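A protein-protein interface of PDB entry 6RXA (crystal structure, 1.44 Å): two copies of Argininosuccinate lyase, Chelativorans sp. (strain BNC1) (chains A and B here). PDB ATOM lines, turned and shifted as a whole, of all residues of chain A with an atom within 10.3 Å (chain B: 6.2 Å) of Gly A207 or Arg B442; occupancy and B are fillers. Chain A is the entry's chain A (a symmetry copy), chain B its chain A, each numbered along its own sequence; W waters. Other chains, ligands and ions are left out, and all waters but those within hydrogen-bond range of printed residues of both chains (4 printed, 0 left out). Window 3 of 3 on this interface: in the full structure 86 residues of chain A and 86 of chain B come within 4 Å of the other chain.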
ATOM      1  N   LEU A  54     -17.945  29.458 -16.296  1.00  0.00           N
ATOM      2  CA  LEU A  54     -17.205  28.284 -16.743  1.00  0.00           C
ATOM      3  C   LEU A  54     -16.010  28.029 -15.843  1.00  0.00           C
ATOM      4  O   LEU A  54     -15.608  26.875 -15.649  1.00  0.00           O
ATOM      5  CB  LEU A  54     -16.703  28.456 -18.168  1.00  0.00           C
ATOM      6  CG  LEU A  54     -17.711  28.533 -19.299  1.00  0.00           C
ATOM      7  CD1 LEU A  54     -16.992  28.697 -20.622  1.00  0.00           C
ATOM      8  CD2 LEU A  54     -18.576  27.289 -19.329  1.00  0.00           C
ATOM      9  N   GLN A  57     -17.113  26.374 -12.674  1.00  0.00           N
ATOM     10  CA  GLN A  57     -17.480  24.993 -12.960  1.00  0.00           C
ATOM     11  C   GLN A  57     -16.283  24.123 -13.325  1.00  0.00           C
ATOM     12  O   GLN A  57     -16.466  22.921 -13.559  1.00  0.00           O
ATOM     13  CB  GLN A  57     -18.518  24.942 -14.083  1.00  0.00           C
ATOM     14  CG  GLN A  57     -19.825  25.613 -13.737  1.00  0.00           C
ATOM     15  CD  GLN A  57     -20.463  25.018 -12.505  1.00  0.00           C
ATOM     16  OE1 GLN A  57     -20.328  25.547 -11.402  1.00  0.00           O
ATOM     17  NE2 GLN A  57     -21.136  23.898 -12.679  1.00  0.00           N
ATOM     18  N   ILE A  59     -14.627  24.197 -16.063  1.00  0.00           N
ATOM     19  CA  ILE A  59     -14.542  23.980 -17.504  1.00  0.00           C
ATOM     20  C   ILE A  59     -13.355  24.737 -18.079  1.00  0.00           C
ATOM     21  O   ILE A  59     -12.659  24.245 -18.978  1.00  0.00           O
ATOM     22  CB  ILE A  59     -15.878  24.363 -18.166  1.00  0.00           C
ATOM     23  CG1 ILE A  59     -16.966  23.392 -17.686  1.00  0.00           C
ATOM     24  CG2 ILE A  59     -15.762  24.345 -19.668  1.00  0.00           C
ATOM     25  CD1 ILE A  59     -18.372  23.802 -18.051  1.00  0.00           C
ATOM     26  N   ILE A 108     -17.823  27.549 -25.293  1.00  0.00           N
ATOM     27  CA  ILE A 108     -18.212  26.241 -24.778  1.00  0.00           C
ATOM     28  C   ILE A 108     -19.567  26.331 -24.088  1.00  0.00           C
ATOM     29  O   ILE A 108     -19.791  27.182 -23.215  1.00  0.00           O
ATOM     30  CB  ILE A 108     -17.123  25.695 -23.839  1.00  0.00           C
ATOM     31  CG1 ILE A 108     -15.895  25.270 -24.647  1.00  0.00           C
ATOM     32  CG2 ILE A 108     -17.677  24.533 -23.027  1.00  0.00           C
ATOM     33  CD1 ILE A 108     -14.661  24.970 -23.784  1.00  0.00           C
ATOM     34  N   GLY A 109     -20.479  25.444 -24.470  1.00  0.00           N
ATOM     35  CA  GLY A 109     -21.784  25.381 -23.842  1.00  0.00           C
ATOM     36  C   GLY A 109     -22.747  26.492 -24.205  1.00  0.00           C
ATOM     37  O   GLY A 109     -23.763  26.652 -23.532  1.00  0.00           O
ATOM     38  N   ARG A 110     -22.479  27.244 -25.272  1.00  0.00           N
ATOM     39  CA  ARG A 110     -23.230  28.449 -25.602  1.00  0.00           C
ATOM     40  C   ARG A 110     -23.465  28.505 -27.103  1.00  0.00           C
ATOM     41  O   ARG A 110     -22.861  27.762 -27.881  1.00  0.00           O
ATOM     42  CB  ARG A 110     -22.438  29.687 -25.132  1.00  0.00           C
ATOM     43  CG  ARG A 110     -23.158  30.997 -25.200  1.00  0.00           C
ATOM     44  CD  ARG A 110     -22.280  32.094 -24.614  1.00  0.00           C
ATOM     45  NE  ARG A 110     -21.065  32.338 -25.382  1.00  0.00           N
ATOM     46  CZ  ARG A 110     -20.326  33.433 -25.231  1.00  0.00           C
ATOM     47  NH1 ARG A 110     -20.706  34.354 -24.361  1.00  0.00           N
ATOM     48  NH2 ARG A 110     -19.237  33.624 -25.960  1.00  0.00           N
ATOM     49  N   GLY A 199     -27.735  29.237 -21.118  1.00  0.00           N
ATOM     50  CA  GLY A 199     -27.735  27.822 -20.809  1.00  0.00           C
ATOM     51  C   GLY A 199     -28.619  27.028 -21.738  1.00  0.00           C
ATOM     52  O   GLY A 199     -28.481  25.795 -21.811  1.00  0.00           O
ATOM     53  N   ALA A 200     -29.522  27.697 -22.455  1.00  0.00           N
ATOM     54  CA  ALA A 200     -30.277  27.037 -23.510  1.00  0.00           C
ATOM     55  C   ALA A 200     -29.394  26.680 -24.697  1.00  0.00           C
ATOM     56  O   ALA A 200     -29.752  25.800 -25.490  1.00  0.00           O
ATOM     57  CB  ALA A 200     -31.404  27.955 -23.983  1.00  0.00           C
ATOM     58  N   ALA A 201     -28.249  27.342 -24.835  1.00  0.00           N
ATOM     59  CA  ALA A 201     -27.330  27.115 -25.956  1.00  0.00           C
ATOM     60  C   ALA A 201     -28.112  27.260 -27.263  1.00  0.00           C
ATOM     61  O   ALA A 201     -28.777  28.286 -27.457  1.00  0.00           O
ATOM     62  CB  ALA A 201     -26.551  25.822 -25.765  1.00  0.00           C
ATOM     63  N   ALA A 202     -28.057  26.279 -28.173  1.00  0.00           N
ATOM     64  CA  ALA A 202     -28.712  26.429 -29.465  1.00  0.00           C
ATOM     65  C   ALA A 202     -30.226  26.448 -29.340  1.00  0.00           C
ATOM     66  O   ALA A 202     -30.902  27.121 -30.129  1.00  0.00           O
ATOM     67  CB  ALA A 202     -28.297  25.283 -30.385  1.00  0.00           C
ATOM     68  N   ALA A 204     -31.435  23.441 -27.030  1.00  0.00           N
ATOM     69  CA  ALA A 204     -31.624  22.169 -26.334  1.00  0.00           C
ATOM     70  C   ALA A 204     -30.695  22.008 -25.135  1.00  0.00           C
ATOM     71  O   ALA A 204     -30.514  20.894 -24.642  1.00  0.00           O
ATOM     72  CB  ALA A 204     -31.449  20.985 -27.296  1.00  0.00           C
ATOM     73  N   GLY A 205     -30.101  23.090 -24.642  1.00  0.00           N
ATOM     74  CA  GLY A 205     -29.130  22.935 -23.586  1.00  0.00           C
ATOM     75  C   GLY A 205     -27.831  22.338 -24.097  1.00  0.00           C
ATOM     76  O   GLY A 205     -27.469  22.475 -25.270  1.00  0.00           O
ATOM     77  N   THR A 206     -27.121  21.671 -23.199  1.00  0.00           N
ATOM     78  CA  THR A 206     -25.765  21.231 -23.479  1.00  0.00           C
ATOM     79  C   THR A 206     -25.387  20.139 -22.499  1.00  0.00           C
ATOM     80  O   THR A 206     -25.918  20.072 -21.389  1.00  0.00           O
ATOM     81  CB  THR A 206     -24.778  22.406 -23.375  1.00  0.00           C
ATOM     82  OG1 THR A 206     -23.441  21.938 -23.585  1.00  0.00           O
ATOM     83  CG2 THR A 206     -24.843  23.061 -22.012  1.00  0.00           C
ATOM     84  N   GLY A 207     -24.453  19.293 -22.920  1.00  0.00           N
ATOM     85  CA  GLY A 207     -23.856  18.336 -22.010  1.00  0.00           C
ATOM     86  C   GLY A 207     -22.797  18.904 -21.092  1.00  0.00           C
ATOM     87  O   GLY A 207     -22.397  18.229 -20.137  1.00  0.00           O
ATOM     88  N   TRP A 208     -22.331  20.129 -21.340  1.00  0.00           N
ATOM     89  CA  TRP A 208     -21.386  20.749 -20.424  1.00  0.00           C
ATOM     90  C   TRP A 208     -22.087  21.102 -19.114  1.00  0.00           C
ATOM     91  O   TRP A 208     -23.235  21.555 -19.130  1.00  0.00           O
ATOM     92  CB  TRP A 208     -20.778  22.007 -21.052  1.00  0.00           C
ATOM     93  CG  TRP A 208     -19.857  21.701 -22.183  1.00  0.00           C
ATOM     94  CD1 TRP A 208     -20.146  21.753 -23.514  1.00  0.00           C
ATOM     95  CD2 TRP A 208     -18.500  21.281 -22.078  1.00  0.00           C
ATOM     96  NE1 TRP A 208     -19.046  21.385 -24.249  1.00  0.00           N
ATOM     97  CE2 TRP A 208     -18.021  21.090 -23.390  1.00  0.00           C
ATOM     98  CE3 TRP A 208     -17.638  21.044 -21.003  1.00  0.00           C
ATOM     99  CZ2 TRP A 208     -16.717  20.676 -23.653  1.00  0.00           C
ATOM    100  CZ3 TRP A 208     -16.341  20.632 -21.264  1.00  0.00           C
ATOM    101  CH2 TRP A 208     -15.893  20.456 -22.581  1.00  0.00           C
ATOM    102  N   PRO A 209     -21.421  20.919 -17.968  1.00  0.00           N
ATOM    103  CA  PRO A 209     -22.111  21.128 -16.675  1.00  0.00           C
ATOM    104  C   PRO A 209     -22.161  22.596 -16.261  1.00  0.00           C
ATOM    105  O   PRO A 209     -21.485  23.055 -15.341  1.00  0.00           O
ATOM    106  CB  PRO A 209     -21.281  20.263 -15.718  1.00  0.00           C
ATOM    107  CG  PRO A 209     -19.908  20.304 -16.285  1.00  0.00           C
ATOM    108  CD  PRO A 209     -20.081  20.329 -17.796  1.00  0.00           C
ATOM    109  N   LEU A 210     -23.009  23.362 -16.938  1.00  0.00           N
ATOM    110  CA  LEU A 210     -23.140  24.774 -16.615  1.00  0.00           C
ATOM    111  C   LEU A 210     -23.899  24.943 -15.305  1.00  0.00           C
ATOM    112  O   LEU A 210     -24.689  24.084 -14.895  1.00  0.00           O
ATOM    113  CB  LEU A 210     -23.900  25.493 -17.727  1.00  0.00           C
ATOM    114  CG  LEU A 210     -23.412  25.241 -19.160  1.00  0.00           C
ATOM    115  CD1 LEU A 210     -24.181  26.137 -20.131  1.00  0.00           C
ATOM    116  CD2 LEU A 210     -21.905  25.452 -19.292  1.00  0.00           C
ATOM    117  N   ASN A 211     -23.670  26.073 -14.655  1.00  0.00           N
ATOM    118  CA  ASN A 211     -24.498  26.521 -13.539  1.00  0.00           C
ATOM    119  C   ASN A 211     -25.295  27.722 -14.041  1.00  0.00           C
ATOM    120  O   ASN A 211     -24.805  28.860 -14.024  1.00  0.00           O
ATOM    121  CB  ASN A 211     -23.671  26.874 -12.311  1.00  0.00           C
ATOM    122  CG  ASN A 211     -24.534  27.285 -11.135  1.00  0.00           C
ATOM    123  OD1 ASN A 211     -25.733  27.526 -11.283  1.00  0.00           O
ATOM    124  ND2 ASN A 211     -23.924  27.381  -9.961  1.00  0.00           N
ATOM    125  N   SER A 228     -35.280  25.192 -22.464  1.00  0.00           N
ATOM    126  CA  SER A 228     -34.265  25.672 -23.400  1.00  0.00           C
ATOM    127  C   SER A 228     -34.861  26.142 -24.721  1.00  0.00           C
ATOM    128  O   SER A 228     -34.321  27.069 -25.339  1.00  0.00           O
ATOM    129  CB  SER A 228     -33.223  24.589 -23.656  1.00  0.00           C
ATOM    130  OG  SER A 228     -33.823  23.421 -24.188  1.00  0.00           O
ATOM    131  N   ASP B 369     -22.714  17.129 -30.311  1.00  0.00           N
ATOM    132  CA  ASP B 369     -22.109  16.243 -29.322  1.00  0.00           C
ATOM    133  C   ASP B 369     -20.776  15.687 -29.803  1.00  0.00           C
ATOM    134  O   ASP B 369     -19.848  15.512 -29.008  1.00  0.00           O
ATOM    135  CB  ASP B 369     -23.060  15.130 -28.912  1.00  0.00           C
ATOM    136  CG  ASP B 369     -23.963  15.557 -27.780  1.00  0.00           C
ATOM    137  OD1 ASP B 369     -24.106  16.785 -27.594  1.00  0.00           O
ATOM    138  OD2 ASP B 369     -24.508  14.683 -27.067  1.00  0.00           O
ATOM    139  N   ASP B 372     -18.410  18.653 -29.149  1.00  0.00           N
ATOM    140  CA  ASP B 372     -18.141  18.809 -27.725  1.00  0.00           C
ATOM    141  C   ASP B 372     -17.217  17.709 -27.226  1.00  0.00           C
ATOM    142  O   ASP B 372     -16.380  17.944 -26.341  1.00  0.00           O
ATOM    143  CB  ASP B 372     -19.448  18.741 -26.931  1.00  0.00           C
ATOM    144  CG  ASP B 372     -20.263  20.030 -26.977  1.00  0.00           C
ATOM    145  OD1 ASP B 372     -19.687  21.129 -27.078  1.00  0.00           O
ATOM    146  OD2 ASP B 372     -21.501  19.936 -26.874  1.00  0.00           O
ATOM    147  N   ARG B 376     -13.734  18.154 -25.228  1.00  0.00           N
ATOM    148  CA  ARG B 376     -13.613  17.569 -23.898  1.00  0.00           C
ATOM    149  C   ARG B 376     -12.495  16.536 -23.842  1.00  0.00           C
ATOM    150  O   ARG B 376     -11.767  16.463 -22.844  1.00  0.00           O
ATOM    151  CB  ARG B 376     -14.951  16.931 -23.520  1.00  0.00           C
ATOM    152  CG  ARG B 376     -15.088  16.525 -22.068  1.00  0.00           C
ATOM    153  CD  ARG B 376     -16.451  15.870 -21.811  1.00  0.00           C
ATOM    154  NE  ARG B 376     -17.570  16.804 -21.966  1.00  0.00           N
ATOM    155  CZ  ARG B 376     -18.467  16.775 -22.954  1.00  0.00           C
ATOM    156  NH1 ARG B 376     -18.408  15.853 -23.910  1.00  0.00           N
ATOM    157  NH2 ARG B 376     -19.436  17.682 -22.981  1.00  0.00           N
ATOM    158  N   ASP B 432     -20.624   6.833 -29.107  1.00  0.00           N
ATOM    159  CA  ASP B 432     -21.436   7.375 -28.022  1.00  0.00           C
ATOM    160  C   ASP B 432     -21.843   8.818 -28.285  1.00  0.00           C
ATOM    161  O   ASP B 432     -22.919   9.243 -27.856  1.00  0.00           O
ATOM    162  CB  ASP B 432     -20.673   7.269 -26.702  1.00  0.00           C
ATOM    163  CG  ASP B 432     -21.436   7.873 -25.544  1.00  0.00           C
ATOM    164  OD1 ASP B 432     -22.526   7.360 -25.210  1.00  0.00           O
ATOM    165  OD2 ASP B 432     -20.943   8.866 -24.968  1.00  0.00           O
ATOM    166  N   ALA B 433     -21.000   9.589 -28.975  1.00  0.00           N
ATOM    167  CA  ALA B 433     -21.363  10.961 -29.302  1.00  0.00           C
ATOM    168  C   ALA B 433     -22.491  11.011 -30.324  1.00  0.00           C
ATOM    169  O   ALA B 433     -23.291  11.953 -30.320  1.00  0.00           O
ATOM    170  CB  ALA B 433     -20.140  11.711 -29.830  1.00  0.00           C
ATOM    171  N   LEU B 434     -22.578  10.005 -31.196  1.00  0.00           N
ATOM    172  CA  LEU B 434     -23.556   9.993 -32.277  1.00  0.00           C
ATOM    173  C   LEU B 434     -24.852   9.286 -31.909  1.00  0.00           C
ATOM    174  O   LEU B 434     -25.771   9.228 -32.736  1.00  0.00           O
ATOM    175  CB  LEU B 434     -22.963   9.309 -33.512  1.00  0.00           C
ATOM    176  CG  LEU B 434     -21.721   9.946 -34.118  1.00  0.00           C
ATOM    177  CD1 LEU B 434     -21.180   9.057 -35.244  1.00  0.00           C
ATOM    178  CD2 LEU B 434     -21.997  11.339 -34.634  1.00  0.00           C
ATOM    179  N   ASP B 435     -24.955   8.748 -30.707  1.00  0.00           N
ATOM    180  CA  ASP B 435     -26.165   8.061 -30.276  1.00  0.00           C
ATOM    181  C   ASP B 435     -27.170   9.125 -29.860  1.00  0.00           C
ATOM    182  O   ASP B 435     -26.922   9.847 -28.883  1.00  0.00           O
ATOM    183  CB  ASP B 435     -25.811   7.160 -29.094  1.00  0.00           C
ATOM    184  CG  ASP B 435     -27.004   6.396 -28.555  1.00  0.00           C
ATOM    185  OD1 ASP B 435     -28.148   6.878 -28.660  1.00  0.00           O
ATOM    186  OD2 ASP B 435     -26.788   5.300 -27.991  1.00  0.00           O
ATOM    187  N   TRP B 437     -30.024   9.117 -28.341  1.00  0.00           N
ATOM    188  CA  TRP B 437     -30.553   9.014 -26.989  1.00  0.00           C
ATOM    189  C   TRP B 437     -29.515   9.471 -25.972  1.00  0.00           C
ATOM    190  O   TRP B 437     -29.862  10.134 -24.987  1.00  0.00           O
ATOM    191  CB  TRP B 437     -31.017   7.588 -26.690  1.00  0.00           C
ATOM    192  CG  TRP B 437     -31.677   7.470 -25.342  1.00  0.00           C
ATOM    193  CD1 TRP B 437     -31.301   6.669 -24.302  1.00  0.00           C
ATOM    194  CD2 TRP B 437     -32.816   8.206 -24.886  1.00  0.00           C
ATOM    195  NE1 TRP B 437     -32.144   6.855 -23.227  1.00  0.00           N
ATOM    196  CE2 TRP B 437     -33.087   7.792 -23.567  1.00  0.00           C
ATOM    197  CE3 TRP B 437     -33.643   9.175 -25.472  1.00  0.00           C
ATOM    198  CZ2 TRP B 437     -34.143   8.313 -22.823  1.00  0.00           C
ATOM    199  CZ3 TRP B 437     -34.688   9.686 -24.730  1.00  0.00           C
ATOM    200  CH2 TRP B 437     -34.929   9.257 -23.423  1.00  0.00           C
ATOM    201  N   GLN B 438     -28.237   9.143 -26.202  1.00  0.00           N
ATOM    202  CA  GLN B 438     -27.186   9.681 -25.339  1.00  0.00           C
ATOM    203  C   GLN B 438     -27.092  11.199 -25.450  1.00  0.00           C
ATOM    204  O   GLN B 438     -26.736  11.866 -24.472  1.00  0.00           O
ATOM    205  CB  GLN B 438     -25.834   9.024 -25.615  1.00  0.00           C
ATOM    206  CG  GLN B 438     -25.807   7.536 -25.316  1.00  0.00           C
ATOM    207  CD  GLN B 438     -26.169   7.206 -23.880  1.00  0.00           C
ATOM    208  OE1 GLN B 438     -25.639   7.795 -22.939  1.00  0.00           O
ATOM    209  NE2 GLN B 438     -27.082   6.261 -23.708  1.00  0.00           N
ATOM    210  N   ASN B 439     -27.392  11.769 -26.629  1.00  0.00           N
ATOM    211  CA  ASN B 439     -27.431  13.227 -26.735  1.00  0.00           C
ATOM    212  C   ASN B 439     -28.478  13.790 -25.780  1.00  0.00           C
ATOM    213  O   ASN B 439     -28.269  14.836 -25.151  1.00  0.00           O
ATOM    214  CB  ASN B 439     -27.786  13.679 -28.159  1.00  0.00           C
ATOM    215  CG  ASN B 439     -26.604  13.705 -29.093  1.00  0.00           C
ATOM    216  OD1 ASN B 439     -26.340  14.721 -29.735  1.00  0.00           O
ATOM    217  ND2 ASN B 439     -25.914  12.590 -29.207  1.00  0.00           N
ATOM    218  N   VAL B 440     -29.637  13.128 -25.696  1.00  0.00           N
ATOM    219  CA  VAL B 440     -30.696  13.583 -24.803  1.00  0.00           C
ATOM    220  C   VAL B 440     -30.265  13.430 -23.355  1.00  0.00           C
ATOM    221  O   VAL B 440     -30.370  14.366 -22.556  1.00  0.00           O
ATOM    222  CB  VAL B 440     -31.999  12.816 -25.092  1.00  0.00           C
ATOM    223  CG1 VAL B 440     -33.016  13.096 -24.023  1.00  0.00           C
ATOM    224  CG2 VAL B 440     -32.553  13.217 -26.461  1.00  0.00           C
ATOM    225  N   LEU B 441     -29.735  12.254 -23.004  1.00  0.00           N
ATOM    226  CA  LEU B 441     -29.358  11.990 -21.620  1.00  0.00           C
ATOM    227  C   LEU B 441     -28.273  12.943 -21.135  1.00  0.00           C
ATOM    228  O   LEU B 441     -28.261  13.335 -19.959  1.00  0.00           O
ATOM    229  CB  LEU B 441     -28.902  10.539 -21.479  1.00  0.00           C
ATOM    230  CG  LEU B 441     -29.977   9.472 -21.664  1.00  0.00           C
ATOM    231  CD1 LEU B 441     -29.380   8.070 -21.452  1.00  0.00           C
ATOM    232  CD2 LEU B 441     -31.137   9.714 -20.728  1.00  0.00           C
ATOM    233  N   ARG B 442     -27.333  13.314 -22.008  1.00  0.00           N
ATOM    234  CA  ARG B 442     -26.278  14.236 -21.599  1.00  0.00           C
ATOM    235  C   ARG B 442     -26.803  15.639 -21.311  1.00  0.00           C
ATOM    236  O   ARG B 442     -26.171  16.375 -20.544  1.00  0.00           O
ATOM    237  CB  ARG B 442     -25.191  14.304 -22.676  1.00  0.00           C
ATOM    238  CG  ARG B 442     -24.242  13.125 -22.618  1.00  0.00           C
ATOM    239  CD  ARG B 442     -23.066  13.309 -23.546  1.00  0.00           C
ATOM    240  NE  ARG B 442     -23.431  13.122 -24.945  1.00  0.00           N
ATOM    241  CZ  ARG B 442     -23.343  11.962 -25.597  1.00  0.00           C
ATOM    242  NH1 ARG B 442     -22.891  10.871 -24.991  1.00  0.00           N
ATOM    243  NH2 ARG B 442     -23.697  11.899 -26.874  1.00  0.00           N
ATOM    244  N   ARG B 443     -27.933  16.022 -21.898  1.00  0.00           N
ATOM    245  CA  ARG B 443     -28.501  17.360 -21.719  1.00  0.00           C
ATOM    246  C   ARG B 443     -29.456  17.313 -20.530  1.00  0.00           C
ATOM    247  O   ARG B 443     -30.683  17.288 -20.675  1.00  0.00           O
ATOM    248  CB  ARG B 443     -29.187  17.813 -23.000  1.00  0.00           C
ATOM    249  CG  ARG B 443     -28.218  18.099 -24.142  1.00  0.00           C
ATOM    250  CD  ARG B 443     -28.937  18.245 -25.485  1.00  0.00           C
ATOM    251  NE  ARG B 443     -28.009  18.822 -26.455  1.00  0.00           N
ATOM    252  CZ  ARG B 443     -26.982  18.164 -26.982  1.00  0.00           C
ATOM    253  NH1 ARG B 443     -26.154  18.770 -27.829  1.00  0.00           N
ATOM    254  NH2 ARG B 443     -26.777  16.894 -26.661  1.00  0.00           N
ATOM    255  N   GLU B 444     -28.864  17.311 -19.329  1.00  0.00           N
ATOM    256  CA  GLU B 444     -29.599  17.032 -18.098  1.00  0.00           C
ATOM    257  C   GLU B 444     -29.744  18.226 -17.153  1.00  0.00           C
ATOM    258  O   GLU B 444     -30.244  18.054 -16.037  1.00  0.00           O
ATOM    259  CB  GLU B 444     -28.978  15.839 -17.364  1.00  0.00           C
ATOM    260  CG  GLU B 444     -27.505  16.015 -17.040  1.00  0.00           C
ATOM    261  CD  GLU B 444     -26.958  14.864 -16.220  1.00  0.00           C
ATOM    262  OE1 GLU B 444     -25.753  14.887 -15.889  1.00  0.00           O
ATOM    263  OE2 GLU B 444     -27.740  13.940 -15.910  1.00  0.00           O
ATOM    264  N   GLY B 445     -29.372  19.428 -17.564  1.00  0.00           N
ATOM    265  CA  GLY B 445     -29.572  20.591 -16.726  1.00  0.00           C
ATOM    266  C   GLY B 445     -31.012  21.105 -16.721  1.00  0.00           C
ATOM    267  O   GLY B 445     -31.933  20.527 -17.309  1.00  0.00           O
ATOM    268  N   MET B 448     -33.607  21.255 -19.922  1.00  0.00           N
ATOM    269  CA  MET B 448     -33.002  20.465 -20.984  1.00  0.00           C
ATOM    270  C   MET B 448     -33.777  19.167 -21.162  1.00  0.00           C
ATOM    271  O   MET B 448     -34.617  18.806 -20.335  1.00  0.00           O
ATOM    272  CB  MET B 448     -31.536  20.234 -20.638  1.00  0.00           C
ATOM    273  CG  MET B 448     -30.807  21.561 -20.429  1.00  0.00           C
ATOM    274  SD  MET B 448     -29.036  21.333 -20.233  1.00  0.00           S
ATOM    275  CE  MET B 448     -28.536  22.958 -19.651  1.00  0.00           C
ATOM    276  N   ALA B 450     -33.269  15.826 -21.114  1.00  0.00           N
ATOM    277  CA  ALA B 450     -33.152  14.551 -20.420  1.00  0.00           C
ATOM    278  C   ALA B 450     -34.433  14.263 -19.638  1.00  0.00           C
ATOM    279  O   ALA B 450     -35.007  15.181 -19.029  1.00  0.00           O
ATOM    280  CB  ALA B 450     -31.974  14.607 -19.444  1.00  0.00           C
HETATM  281  O   HOH W   1     -23.217  18.434 -25.454  1.00  0.00           O
HETATM  282  O   HOH W   2     -20.793  23.680 -26.768  1.00  0.00           O
HETATM  283  O   HOH W   3     -23.009  22.078 -26.294  1.00  0.00           O
HETATM  284  O   HOH W   4     -25.556  21.723 -27.162  1.00  0.00           O
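OD1 of Asp B372 lies within hydrogen-bond range of NE1 of Trp A208 (2.9 Å).
The side-chain sulfur of Met B448 lies within hydrogen-bond range of the backbone NH of Thr A206, 3.5 Å away.
The guanidinium group (NH2) of Arg B442 lies within hydrogen-bond range of the backbone carbonyl oxygen (O) of Ala B433, 3.5 Å away.
The backbone NH (N) of Ala B450 is in hydrogen-bond range of the backbone carbonyl oxygen (O) of Arg B443, 3.0 Å away.
The side-chain carboxylate (OD2) of Asp B432 is in salt-bridge range of the guanidinium group (NH1) of Arg B442, 2.8 Å away.
The backbone carbonyl oxygen (O) of Ala A200 lies within hydrogen-bond range of the backbone NH (N) of Gly A205, at 2.9 Å.
The side-chain carboxylate of Asp B369 is in salt-bridge range of the guanidinium group of Arg B443.
N of Gly B445 sits at hydrogen-bond distance from SD of Met B448 (3.3 Å).
Of the printed residues of chain B, Gly A199 touches Met B448 (3.6 Å).
No residue of chain A comes within 4 Å of Asp B432.
No residue of chain A comes within 4 Å of Ala B433.
No residue of chain A comes within 4 Å of Asn B439.
Arg B442 touches two residues of chain A.
Arg B443 touches three residues of chain A.
Printed residues of chain A within 4 Å of Met B448: Gly A199, Gly A205 and Thr A206.
The nearest residue of chain B that does not touch Gly A207 is Arg B376 (4.04 Å).
No position is printed for both chains.
Of the 10 pairs that touch across the chains among the printed residues, none has its exchanged pair printed and touching as well.
Water W3 bridges OD2 of Asp B372 (2.7 Å) and OG1 of Thr A206 (2.7 Å).
Water W1 lies within hydrogen-bond range of OD2 of Asp B372, OD1 of Asp B369 and N of Gly A207.
Water W4 bridges O of Gly A205 (2.8 Å) and NH1 of Arg B443 (3.1 Å).
Water W2 bridges OD1 of Asp B372 (2.8 Å) and N of Gly A109 (2.9 Å).
Of the 18 printed residues of chain B, 5 touch a printed residue of chain A.
Printed residues of chain A that touch a printed residue of chain B: Gly A199, Ala A204, Gly A205, Thr A206, Gly A207 and Trp A208.
Among the printed residues, no Asp or Glu carboxylate lies within 4 Å of a Lys or Arg side-chain nitrogen of the other chain.
Met B448 touches Gly A199 (CE to O, 3.6 Å).
CD of Arg B443 touches O of Ala A204 (3.2 Å).
Arg B443 touches Gly A205 (NE to O, 3.9 Å).
Met B448 touches Gly A205 (SD to CA, 3.7 Å).
Arg B442 touches Thr A206.
Thr A206 touches Arg B443.
O of Arg B442 touches CA of Gly A207, at 3.4 Å.
NH2 of Arg B376 touches CE2 of Trp A208, 3.7 Å away.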
